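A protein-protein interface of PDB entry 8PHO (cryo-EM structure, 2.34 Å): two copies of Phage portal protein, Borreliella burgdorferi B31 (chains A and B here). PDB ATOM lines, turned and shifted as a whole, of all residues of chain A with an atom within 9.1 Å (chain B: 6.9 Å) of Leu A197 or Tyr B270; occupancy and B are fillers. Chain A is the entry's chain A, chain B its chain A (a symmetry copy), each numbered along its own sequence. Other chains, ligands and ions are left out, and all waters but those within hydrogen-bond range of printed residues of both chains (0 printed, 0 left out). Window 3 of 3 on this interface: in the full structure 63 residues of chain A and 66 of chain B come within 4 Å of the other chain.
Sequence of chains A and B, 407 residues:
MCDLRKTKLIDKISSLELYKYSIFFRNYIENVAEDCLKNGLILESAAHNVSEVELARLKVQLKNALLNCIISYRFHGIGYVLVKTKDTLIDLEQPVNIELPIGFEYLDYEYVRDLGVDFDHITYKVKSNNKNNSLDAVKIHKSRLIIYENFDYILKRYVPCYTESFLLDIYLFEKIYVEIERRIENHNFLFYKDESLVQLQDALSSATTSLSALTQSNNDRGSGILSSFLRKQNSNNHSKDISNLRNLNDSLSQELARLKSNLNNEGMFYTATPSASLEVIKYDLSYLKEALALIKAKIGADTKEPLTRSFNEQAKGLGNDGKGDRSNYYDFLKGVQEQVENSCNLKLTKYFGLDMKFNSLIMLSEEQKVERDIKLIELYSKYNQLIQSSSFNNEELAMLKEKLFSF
The backbone NH of Asp A194 is in hydrogen-bond range of the backbone carbonyl oxygen of Thr B271 (3.2 Å).
O of Leu A190 is in hydrogen-bond range of N of Phe B269, 2.8 Å away.
N of Tyr A192 lies within hydrogen-bond range of O of Phe B269 (2.9 Å).
The backbone carbonyl oxygen (O) of Tyr A192 lies within hydrogen-bond range of the backbone NH (N) of Thr B271, at 3.2 Å.
The backbone carbonyl oxygen (O) of Asp A194 sits at hydrogen-bond distance from the side-chain hydroxyl (OH) of Tyr B270 (2.8 Å).
OH of Tyr B192 is in hydrogen-bond range of OG1 of Thr B271.
The side-chain hydroxyl (OG1) of Thr A271 lies within hydrogen-bond range of the side-chain carboxylate (OD2) of Asp A194 (3.2 Å).
The side-chain hydroxyl of Thr B271 sits at hydrogen-bond distance from the side-chain carboxylate of Asp B194.
O of Ser A277 lies within hydrogen-bond range of N of Lys A193, 3.1 Å away.
The side-chain hydroxyl (OG1) of Thr A273 is in hydrogen-bond range of the side-chain carboxylate (OD1) of Asp A194 (2.8 Å).
The side-chain hydroxyl (OH) of Tyr A192 is in hydrogen-bond range of the side-chain carboxylate (OD2) of Asp A194 (2.6 Å).
Among the printed residues, merely in contact across the chains: Leu A190 with Met B268 (3.6 Å), Phe A191 with Phe B269 (3.4 Å), Phe A191 with Thr B271 (3.9 Å), Tyr A192 with Tyr B270 (3.5 Å), Lys A193 with Thr B271 (3.6 Å), Asp A194 with Ala B272 (3.7 Å), Glu A195 with Ala B272 (3.5 Å) and Leu A197 with Tyr B270 (3.1 Å).
Of chain B, only Tyr B270 comes within 4 Å of Leu A197.
Tyr B270 touches just these residues of chain A: Tyr A192, Asp A194 and Leu A197.
Of chain A, only Leu A190, Phe A191 and Tyr A192 come within 4 Å of Phe B269.
Of chain A, only Phe A191 (3.9 Å), Tyr A192 (3.2 Å), Lys A193 (3.6 Å) and Asp A194 (3.2 Å) come within 4 Å of Thr B271.
Of the printed residues of chain B, Tyr A192 touches Phe B269 (2.9 Å), Tyr B270 (3.5 Å) and Thr B271 (3.2 Å).
Of the printed residues of chain A, Ala B272 touches Asp A194 (3.7 Å) and Glu A195 (3.5 Å).
The nearest residue of chain B that does not touch Leu A197 is Ala B272 (6.3 Å).
The nearest residue of chain A that does not touch Tyr B270 is Glu A195 (4.6 Å).
Of the 17 printed residues of chain A, 7 touch a printed residue of chain B.
Printed residues of chain A that touch a printed residue of chain B: Leu A190, Phe A191, Tyr A192, Lys A193, Asp A194, Glu A195 and Leu A197.
Hydrophobic or aromatic side chains of chain A within 4 Å of the printed part of chain B: Phe A191, Tyr A192 and Leu A197.
Of the 8 printed residues of chain B, 5 touch a printed residue of chain A.
Hydrophobic or aromatic side chains of chain B that line the printed part of chain A: Phe B269, Tyr B270 and Ala B272.
Among the printed residues, 13 pairs touch across the chains.
Tyr A192 touches Tyr B270, but with the chains exchanged Tyr A270 does not touch Tyr B192 (19.2 Å).
Tyr A192 touches Thr B271, but with the chains exchanged Thr A271 does not touch Tyr B192 (16.7 Å).
Asp A194 touches Thr B271, but with the chains exchanged Thr A271 does not touch Asp B194 (17.1 Å).
Asp A194 touches Ala B272, but with the chains exchanged Ala A272 does not touch Asp B194 (19.2 Å).
Positions printed for both chains: 192, 194, 269, 270, 271 and 272.
Of the 13 pairs that touch across the chains among the printed residues, none has its exchanged pair printed and touching as well.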
ATOM      1  N   PHE A 189      35.241 -10.068 -18.583  1.00  0.00           N
ATOM      2  CA  PHE A 189      34.818  -9.423 -17.340  1.00  0.00           C
ATOM      3  C   PHE A 189      34.380 -10.491 -16.347  1.00  0.00           C
ATOM      4  O   PHE A 189      34.150 -11.645 -16.713  1.00  0.00           O
ATOM      5  CB  PHE A 189      33.698  -8.390 -17.559  1.00  0.00           C
ATOM      6  CG  PHE A 189      32.403  -8.967 -18.091  1.00  0.00           C
ATOM      7  CD1 PHE A 189      31.417  -9.425 -17.228  1.00  0.00           C
ATOM      8  CD2 PHE A 189      32.199  -9.098 -19.452  1.00  0.00           C
ATOM      9  CE1 PHE A 189      30.246  -9.976 -17.716  1.00  0.00           C
ATOM     10  CE2 PHE A 189      31.032  -9.654 -19.945  1.00  0.00           C
ATOM     11  CZ  PHE A 189      30.034 -10.042 -19.076  1.00  0.00           C
ATOM     12  N   LEU A 190      34.257 -10.090 -15.082  1.00  0.00           N
ATOM     13  CA  LEU A 190      33.954 -11.008 -13.989  1.00  0.00           C
ATOM     14  C   LEU A 190      32.465 -11.002 -13.663  1.00  0.00           C
ATOM     15  O   LEU A 190      31.828  -9.946 -13.633  1.00  0.00           O
ATOM     16  CB  LEU A 190      34.756 -10.649 -12.735  1.00  0.00           C
ATOM     17  CG  LEU A 190      36.269 -10.856 -12.804  1.00  0.00           C
ATOM     18  CD1 LEU A 190      36.955 -10.128 -11.664  1.00  0.00           C
ATOM     19  CD2 LEU A 190      36.603 -12.339 -12.765  1.00  0.00           C
ATOM     20  N   PHE A 191      31.916 -12.191 -13.421  1.00  0.00           N
ATOM     21  CA  PHE A 191      30.530 -12.372 -12.999  1.00  0.00           C
ATOM     22  C   PHE A 191      30.555 -12.869 -11.558  1.00  0.00           C
ATOM     23  O   PHE A 191      30.933 -14.015 -11.296  1.00  0.00           O
ATOM     24  CB  PHE A 191      29.801 -13.348 -13.921  1.00  0.00           C
ATOM     25  CG  PHE A 191      28.396 -13.646 -13.494  1.00  0.00           C
ATOM     26  CD1 PHE A 191      27.524 -12.617 -13.179  1.00  0.00           C
ATOM     27  CD2 PHE A 191      27.947 -14.953 -13.388  1.00  0.00           C
ATOM     28  CE1 PHE A 191      26.230 -12.879 -12.780  1.00  0.00           C
ATOM     29  CE2 PHE A 191      26.651 -15.221 -12.981  1.00  0.00           C
ATOM     30  CZ  PHE A 191      25.792 -14.179 -12.682  1.00  0.00           C
ATOM     31  N   TYR A 192      30.157 -12.003 -10.629  1.00  0.00           N
ATOM     32  CA  TYR A 192      30.255 -12.272  -9.199  1.00  0.00           C
ATOM     33  C   TYR A 192      28.854 -12.405  -8.613  1.00  0.00           C
ATOM     34  O   TYR A 192      28.007 -11.525  -8.806  1.00  0.00           O
ATOM     35  CB  TYR A 192      31.028 -11.180  -8.484  1.00  0.00           C
ATOM     36  CG  TYR A 192      31.213 -11.410  -7.005  1.00  0.00           C
ATOM     37  CD1 TYR A 192      31.542 -12.676  -6.533  1.00  0.00           C
ATOM     38  CD2 TYR A 192      31.192 -10.366  -6.097  1.00  0.00           C
ATOM     39  CE1 TYR A 192      31.758 -12.921  -5.196  1.00  0.00           C
ATOM     40  CE2 TYR A 192      31.416 -10.599  -4.751  1.00  0.00           C
ATOM     41  CZ  TYR A 192      31.722 -11.870  -4.310  1.00  0.00           C
ATOM     42  OH  TYR A 192      31.937 -12.060  -2.967  1.00  0.00           O
ATOM     43  N   LYS A 193      28.609 -13.516  -7.915  1.00  0.00           N
ATOM     44  CA  LYS A 193      27.351 -13.775  -7.224  1.00  0.00           C
ATOM     45  C   LYS A 193      27.632 -13.908  -5.734  1.00  0.00           C
ATOM     46  O   LYS A 193      28.405 -14.778  -5.322  1.00  0.00           O
ATOM     47  CB  LYS A 193      26.681 -15.043  -7.757  1.00  0.00           C
ATOM     48  CG  LYS A 193      26.391 -15.027  -9.248  1.00  0.00           C
ATOM     49  CD  LYS A 193      25.344 -16.071  -9.580  1.00  0.00           C
ATOM     50  CE  LYS A 193      25.825 -17.451  -9.120  1.00  0.00           C
ATOM     51  NZ  LYS A 193      24.777 -18.454  -9.421  1.00  0.00           N
ATOM     52  N   ASP A 194      27.002 -13.052  -4.931  1.00  0.00           N
ATOM     53  CA  ASP A 194      27.225 -13.056  -3.487  1.00  0.00           C
ATOM     54  C   ASP A 194      25.991 -12.450  -2.835  1.00  0.00           C
ATOM     55  O   ASP A 194      25.716 -11.261  -3.032  1.00  0.00           O
ATOM     56  CB  ASP A 194      28.472 -12.262  -3.134  1.00  0.00           C
ATOM     57  CG  ASP A 194      28.945 -12.528  -1.722  1.00  0.00           C
ATOM     58  OD1 ASP A 194      28.277 -13.297  -0.997  1.00  0.00           O
ATOM     59  OD2 ASP A 194      29.978 -11.951  -1.333  1.00  0.00           O
ATOM     60  N   GLU A 195      25.251 -13.256  -2.072  1.00  0.00           N
ATOM     61  CA  GLU A 195      23.973 -12.782  -1.562  1.00  0.00           C
ATOM     62  C   GLU A 195      24.154 -11.869  -0.358  1.00  0.00           C
ATOM     63  O   GLU A 195      23.485 -10.834  -0.263  1.00  0.00           O
ATOM     64  CB  GLU A 195      23.080 -13.970  -1.212  1.00  0.00           C
ATOM     65  CG  GLU A 195      23.821 -15.093  -0.500  1.00  0.00           C
ATOM     66  CD  GLU A 195      22.937 -16.293  -0.208  1.00  0.00           C
ATOM     67  OE1 GLU A 195      21.731 -16.221  -0.520  1.00  0.00           O
ATOM     68  OE2 GLU A 195      23.438 -17.274   0.380  1.00  0.00           O
ATOM     69  N   SER A 196      25.098 -12.205   0.522  1.00  0.00           N
ATOM     70  CA  SER A 196      25.311 -11.423   1.732  1.00  0.00           C
ATOM     71  C   SER A 196      25.978 -10.084   1.444  1.00  0.00           C
ATOM     72  O   SER A 196      25.733  -9.112   2.166  1.00  0.00           O
ATOM     73  CB  SER A 196      26.139 -12.224   2.730  1.00  0.00           C
ATOM     74  OG  SER A 196      25.604 -13.520   2.943  1.00  0.00           O
ATOM     75  N   LEU A 197      26.821 -10.012   0.416  1.00  0.00           N
ATOM     76  CA  LEU A 197      27.539  -8.778   0.114  1.00  0.00           C
ATOM     77  C   LEU A 197      26.601  -7.708  -0.434  1.00  0.00           C
ATOM     78  O   LEU A 197      26.349  -6.697   0.221  1.00  0.00           O
ATOM     79  CB  LEU A 197      28.670  -9.044  -0.880  1.00  0.00           C
ATOM     80  CG  LEU A 197      29.533  -7.826  -1.215  1.00  0.00           C
ATOM     81  CD1 LEU A 197      30.282  -7.306   0.010  1.00  0.00           C
ATOM     82  CD2 LEU A 197      30.492  -8.098  -2.362  1.00  0.00           C
ATOM     83  N   PHE A 269      41.142 -12.940  -3.708  1.00  0.00           N
ATOM     84  CA  PHE A 269      39.762 -12.497  -3.546  1.00  0.00           C
ATOM     85  C   PHE A 269      39.061 -13.427  -2.562  1.00  0.00           C
ATOM     86  O   PHE A 269      38.990 -14.639  -2.793  1.00  0.00           O
ATOM     87  CB  PHE A 269      39.060 -12.471  -4.907  1.00  0.00           C
ATOM     88  CG  PHE A 269      37.646 -11.977  -4.852  1.00  0.00           C
ATOM     89  CD1 PHE A 269      37.370 -10.626  -4.756  1.00  0.00           C
ATOM     90  CD2 PHE A 269      36.590 -12.861  -4.938  1.00  0.00           C
ATOM     91  CE1 PHE A 269      36.065 -10.177  -4.704  1.00  0.00           C
ATOM     92  CE2 PHE A 269      35.287 -12.423  -4.855  1.00  0.00           C
ATOM     93  CZ  PHE A 269      35.024 -11.078  -4.765  1.00  0.00           C
ATOM     94  N   TYR A 270      38.597 -12.863  -1.448  1.00  0.00           N
ATOM     95  CA  TYR A 270      38.045 -13.620  -0.333  1.00  0.00           C
ATOM     96  C   TYR A 270      36.567 -13.324  -0.125  1.00  0.00           C
ATOM     97  O   TYR A 270      36.124 -12.181  -0.270  1.00  0.00           O
ATOM     98  CB  TYR A 270      38.819 -13.314   0.954  1.00  0.00           C
ATOM     99  CG  TYR A 270      38.191 -13.906   2.191  1.00  0.00           C
ATOM    100  CD1 TYR A 270      38.214 -15.272   2.421  1.00  0.00           C
ATOM    101  CD2 TYR A 270      37.559 -13.092   3.124  1.00  0.00           C
ATOM    102  CE1 TYR A 270      37.637 -15.808   3.552  1.00  0.00           C
ATOM    103  CE2 TYR A 270      36.991 -13.619   4.267  1.00  0.00           C
ATOM    104  CZ  TYR A 270      37.021 -14.979   4.467  1.00  0.00           C
ATOM    105  OH  TYR A 270      36.460 -15.549   5.584  1.00  0.00           O
ATOM    106  N   THR A 271      35.821 -14.367   0.235  1.00  0.00           N
ATOM    107  CA  THR A 271      34.413 -14.266   0.577  1.00  0.00           C
ATOM    108  C   THR A 271      34.086 -15.348   1.595  1.00  0.00           C
ATOM    109  O   THR A 271      34.823 -16.324   1.750  1.00  0.00           O
ATOM    110  CB  THR A 271      33.516 -14.409  -0.654  1.00  0.00           C
ATOM    111  OG1 THR A 271      32.157 -14.116  -0.298  1.00  0.00           O
ATOM    112  CG2 THR A 271      33.574 -15.833  -1.189  1.00  0.00           C
ATOM    113  N   ALA A 272      32.986 -15.141   2.312  1.00  0.00           N
ATOM    114  CA  ALA A 272      32.545 -16.073   3.335  1.00  0.00           C
ATOM    115  C   ALA A 272      31.240 -16.782   2.998  1.00  0.00           C
ATOM    116  O   ALA A 272      30.892 -17.740   3.697  1.00  0.00           O
ATOM    117  CB  ALA A 272      32.406 -15.356   4.686  1.00  0.00           C
ATOM    118  N   THR A 273      30.553 -16.360   1.946  1.00  0.00           N
ATOM    119  CA  THR A 273      29.329 -17.018   1.529  1.00  0.00           C
ATOM    120  C   THR A 273      29.652 -18.366   0.894  1.00  0.00           C
ATOM    121  O   THR A 273      30.509 -18.434   0.011  1.00  0.00           O
ATOM    122  CB  THR A 273      28.577 -16.119   0.554  1.00  0.00           C
ATOM    123  OG1 THR A 273      28.204 -14.923   1.247  1.00  0.00           O
ATOM    124  CG2 THR A 273      27.307 -16.804   0.076  1.00  0.00           C
ATOM    125  N   ALA A 276      28.768 -18.661  -2.953  1.00  0.00           N
ATOM    126  CA  ALA A 276      29.292 -17.607  -3.811  1.00  0.00           C
ATOM    127  C   ALA A 276      29.943 -18.187  -5.065  1.00  0.00           C
ATOM    128  O   ALA A 276      30.460 -19.308  -5.064  1.00  0.00           O
ATOM    129  CB  ALA A 276      30.312 -16.762  -3.051  1.00  0.00           C
ATOM    130  N   SER A 277      29.936 -17.397  -6.143  1.00  0.00           N
ATOM    131  CA  SER A 277      30.551 -17.814  -7.399  1.00  0.00           C
ATOM    132  C   SER A 277      31.342 -16.667  -8.016  1.00  0.00           C
ATOM    133  O   SER A 277      30.984 -15.496  -7.862  1.00  0.00           O
ATOM    134  CB  SER A 277      29.499 -18.313  -8.389  1.00  0.00           C
ATOM    135  OG  SER A 277      28.978 -19.571  -7.999  1.00  0.00           O
ATOM    136  N   LEU A 278      32.384 -17.017  -8.774  1.00  0.00           N
ATOM    137  CA  LEU A 278      33.175 -16.036  -9.518  1.00  0.00           C
ATOM    138  C   LEU A 278      33.616 -16.654 -10.837  1.00  0.00           C
ATOM    139  O   LEU A 278      34.318 -17.670 -10.837  1.00  0.00           O
ATOM    140  CB  LEU A 278      34.384 -15.568  -8.702  1.00  0.00           C
ATOM    141  CG  LEU A 278      35.097 -14.326  -9.251  1.00  0.00           C
ATOM    142  CD1 LEU A 278      34.148 -13.143  -9.372  1.00  0.00           C
ATOM    143  CD2 LEU A 278      36.291 -13.950  -8.397  1.00  0.00           C
ATOM    144  N   TYR B 192      20.888 -13.119 -19.752  1.00  0.00           N
ATOM    145  CA  TYR B 192      20.891 -12.840 -18.322  1.00  0.00           C
ATOM    146  C   TYR B 192      19.562 -13.277 -17.718  1.00  0.00           C
ATOM    147  O   TYR B 192      18.494 -12.888 -18.207  1.00  0.00           O
ATOM    148  CB  TYR B 192      21.142 -11.370 -18.047  1.00  0.00           C
ATOM    149  CG  TYR B 192      21.207 -11.008 -16.583  1.00  0.00           C
ATOM    150  CD1 TYR B 192      21.892 -11.829 -15.694  1.00  0.00           C
ATOM    151  CD2 TYR B 192      20.712  -9.807 -16.107  1.00  0.00           C
ATOM    152  CE1 TYR B 192      22.009 -11.516 -14.358  1.00  0.00           C
ATOM    153  CE2 TYR B 192      20.830  -9.479 -14.768  1.00  0.00           C
ATOM    154  CZ  TYR B 192      21.500 -10.323 -13.905  1.00  0.00           C
ATOM    155  OH  TYR B 192      21.595  -9.961 -12.583  1.00  0.00           O
ATOM    156  N   ASP B 194      17.599 -13.295 -14.037  1.00  0.00           N
ATOM    157  CA  ASP B 194      17.625 -12.735 -12.687  1.00  0.00           C
ATOM    158  C   ASP B 194      16.186 -12.446 -12.287  1.00  0.00           C
ATOM    159  O   ASP B 194      15.543 -11.582 -12.892  1.00  0.00           O
ATOM    160  CB  ASP B 194      18.466 -11.469 -12.647  1.00  0.00           C
ATOM    161  CG  ASP B 194      18.820 -11.055 -11.236  1.00  0.00           C
ATOM    162  OD1 ASP B 194      18.373 -11.728 -10.281  1.00  0.00           O
ATOM    163  OD2 ASP B 194      19.531 -10.045 -11.084  1.00  0.00           O
ATOM    164  N   GLU B 266      34.386  -0.649 -13.824  1.00  0.00           N
ATOM    165  CA  GLU B 266      35.047  -1.588 -12.927  1.00  0.00           C
ATOM    166  C   GLU B 266      35.336  -2.929 -13.587  1.00  0.00           C
ATOM    167  O   GLU B 266      36.314  -3.589 -13.218  1.00  0.00           O
ATOM    168  CB  GLU B 266      34.214  -1.805 -11.659  1.00  0.00           C
ATOM    169  CG  GLU B 266      35.007  -2.442 -10.513  1.00  0.00           C
ATOM    170  CD  GLU B 266      34.163  -2.728  -9.281  1.00  0.00           C
ATOM    171  OE1 GLU B 266      33.481  -3.775  -9.241  1.00  0.00           O
ATOM    172  OE2 GLU B 266      34.128  -1.863  -8.382  1.00  0.00           O
ATOM    173  N   MET B 268      33.315  -5.513 -13.471  1.00  0.00           N
ATOM    174  CA  MET B 268      32.730  -6.572 -12.662  1.00  0.00           C
ATOM    175  C   MET B 268      31.213  -6.464 -12.713  1.00  0.00           C
ATOM    176  O   MET B 268      30.654  -5.389 -12.473  1.00  0.00           O
ATOM    177  CB  MET B 268      33.242  -6.507 -11.213  1.00  0.00           C
ATOM    178  CG  MET B 268      32.655  -7.592 -10.337  1.00  0.00           C
ATOM    179  SD  MET B 268      33.238  -7.514  -8.632  1.00  0.00           S
ATOM    180  CE  MET B 268      34.974  -7.923  -8.826  1.00  0.00           C
ATOM    181  N   PHE B 269      30.551  -7.580 -13.016  1.00  0.00           N
ATOM    182  CA  PHE B 269      29.094  -7.649 -13.014  1.00  0.00           C
ATOM    183  C   PHE B 269      28.641  -8.387 -11.759  1.00  0.00           C
ATOM    184  O   PHE B 269      29.023  -9.543 -11.543  1.00  0.00           O
ATOM    185  CB  PHE B 269      28.604  -8.339 -14.291  1.00  0.00           C
ATOM    186  CG  PHE B 269      27.112  -8.414 -14.408  1.00  0.00           C
ATOM    187  CD1 PHE B 269      26.376  -7.311 -14.797  1.00  0.00           C
ATOM    188  CD2 PHE B 269      26.447  -9.598 -14.166  1.00  0.00           C
ATOM    189  CE1 PHE B 269      25.001  -7.385 -14.901  1.00  0.00           C
ATOM    190  CE2 PHE B 269      25.073  -9.671 -14.238  1.00  0.00           C
ATOM    191  CZ  PHE B 269      24.352  -8.570 -14.631  1.00  0.00           C
ATOM    192  N   TYR B 270      27.873  -7.698 -10.917  1.00  0.00           N
ATOM    193  CA  TYR B 270      27.482  -8.187  -9.602  1.00  0.00           C
ATOM    194  C   TYR B 270      25.979  -8.406  -9.505  1.00  0.00           C
ATOM    195  O   TYR B 270      25.189  -7.626 -10.044  1.00  0.00           O
ATOM    196  CB  TYR B 270      27.933  -7.208  -8.513  1.00  0.00           C
ATOM    197  CG  TYR B 270      27.398  -7.541  -7.143  1.00  0.00           C
ATOM    198  CD1 TYR B 270      27.864  -8.642  -6.441  1.00  0.00           C
ATOM    199  CD2 TYR B 270      26.410  -6.757  -6.557  1.00  0.00           C
ATOM    200  CE1 TYR B 270      27.369  -8.944  -5.190  1.00  0.00           C
ATOM    201  CE2 TYR B 270      25.922  -7.043  -5.298  1.00  0.00           C
ATOM    202  CZ  TYR B 270      26.395  -8.146  -4.627  1.00  0.00           C
ATOM    203  OH  TYR B 270      25.929  -8.476  -3.376  1.00  0.00           O
ATOM    204  N   THR B 271      25.602  -9.466  -8.792  1.00  0.00           N
ATOM    205  CA  THR B 271      24.214  -9.784  -8.500  1.00  0.00           C
ATOM    206  C   THR B 271      24.156 -10.504  -7.163  1.00  0.00           C
ATOM    207  O   THR B 271      25.159 -11.028  -6.674  1.00  0.00           O
ATOM    208  CB  THR B 271      23.584 -10.648  -9.595  1.00  0.00           C
ATOM    209  OG1 THR B 271      22.176 -10.776  -9.358  1.00  0.00           O
ATOM    210  CG2 THR B 271      24.199 -12.041  -9.588  1.00  0.00           C
ATOM    211  N   ALA B 272      22.971 -10.491  -6.560  1.00  0.00           N
ATOM    212  CA  ALA B 272      22.755 -11.122  -5.269  1.00  0.00           C
ATOM    213  C   ALA B 272      21.830 -12.330  -5.325  1.00  0.00           C
ATOM    214  O   ALA B 272      21.750 -13.057  -4.328  1.00  0.00           O
ATOM    215  CB  ALA B 272      22.208 -10.100  -4.260  1.00  0.00           C
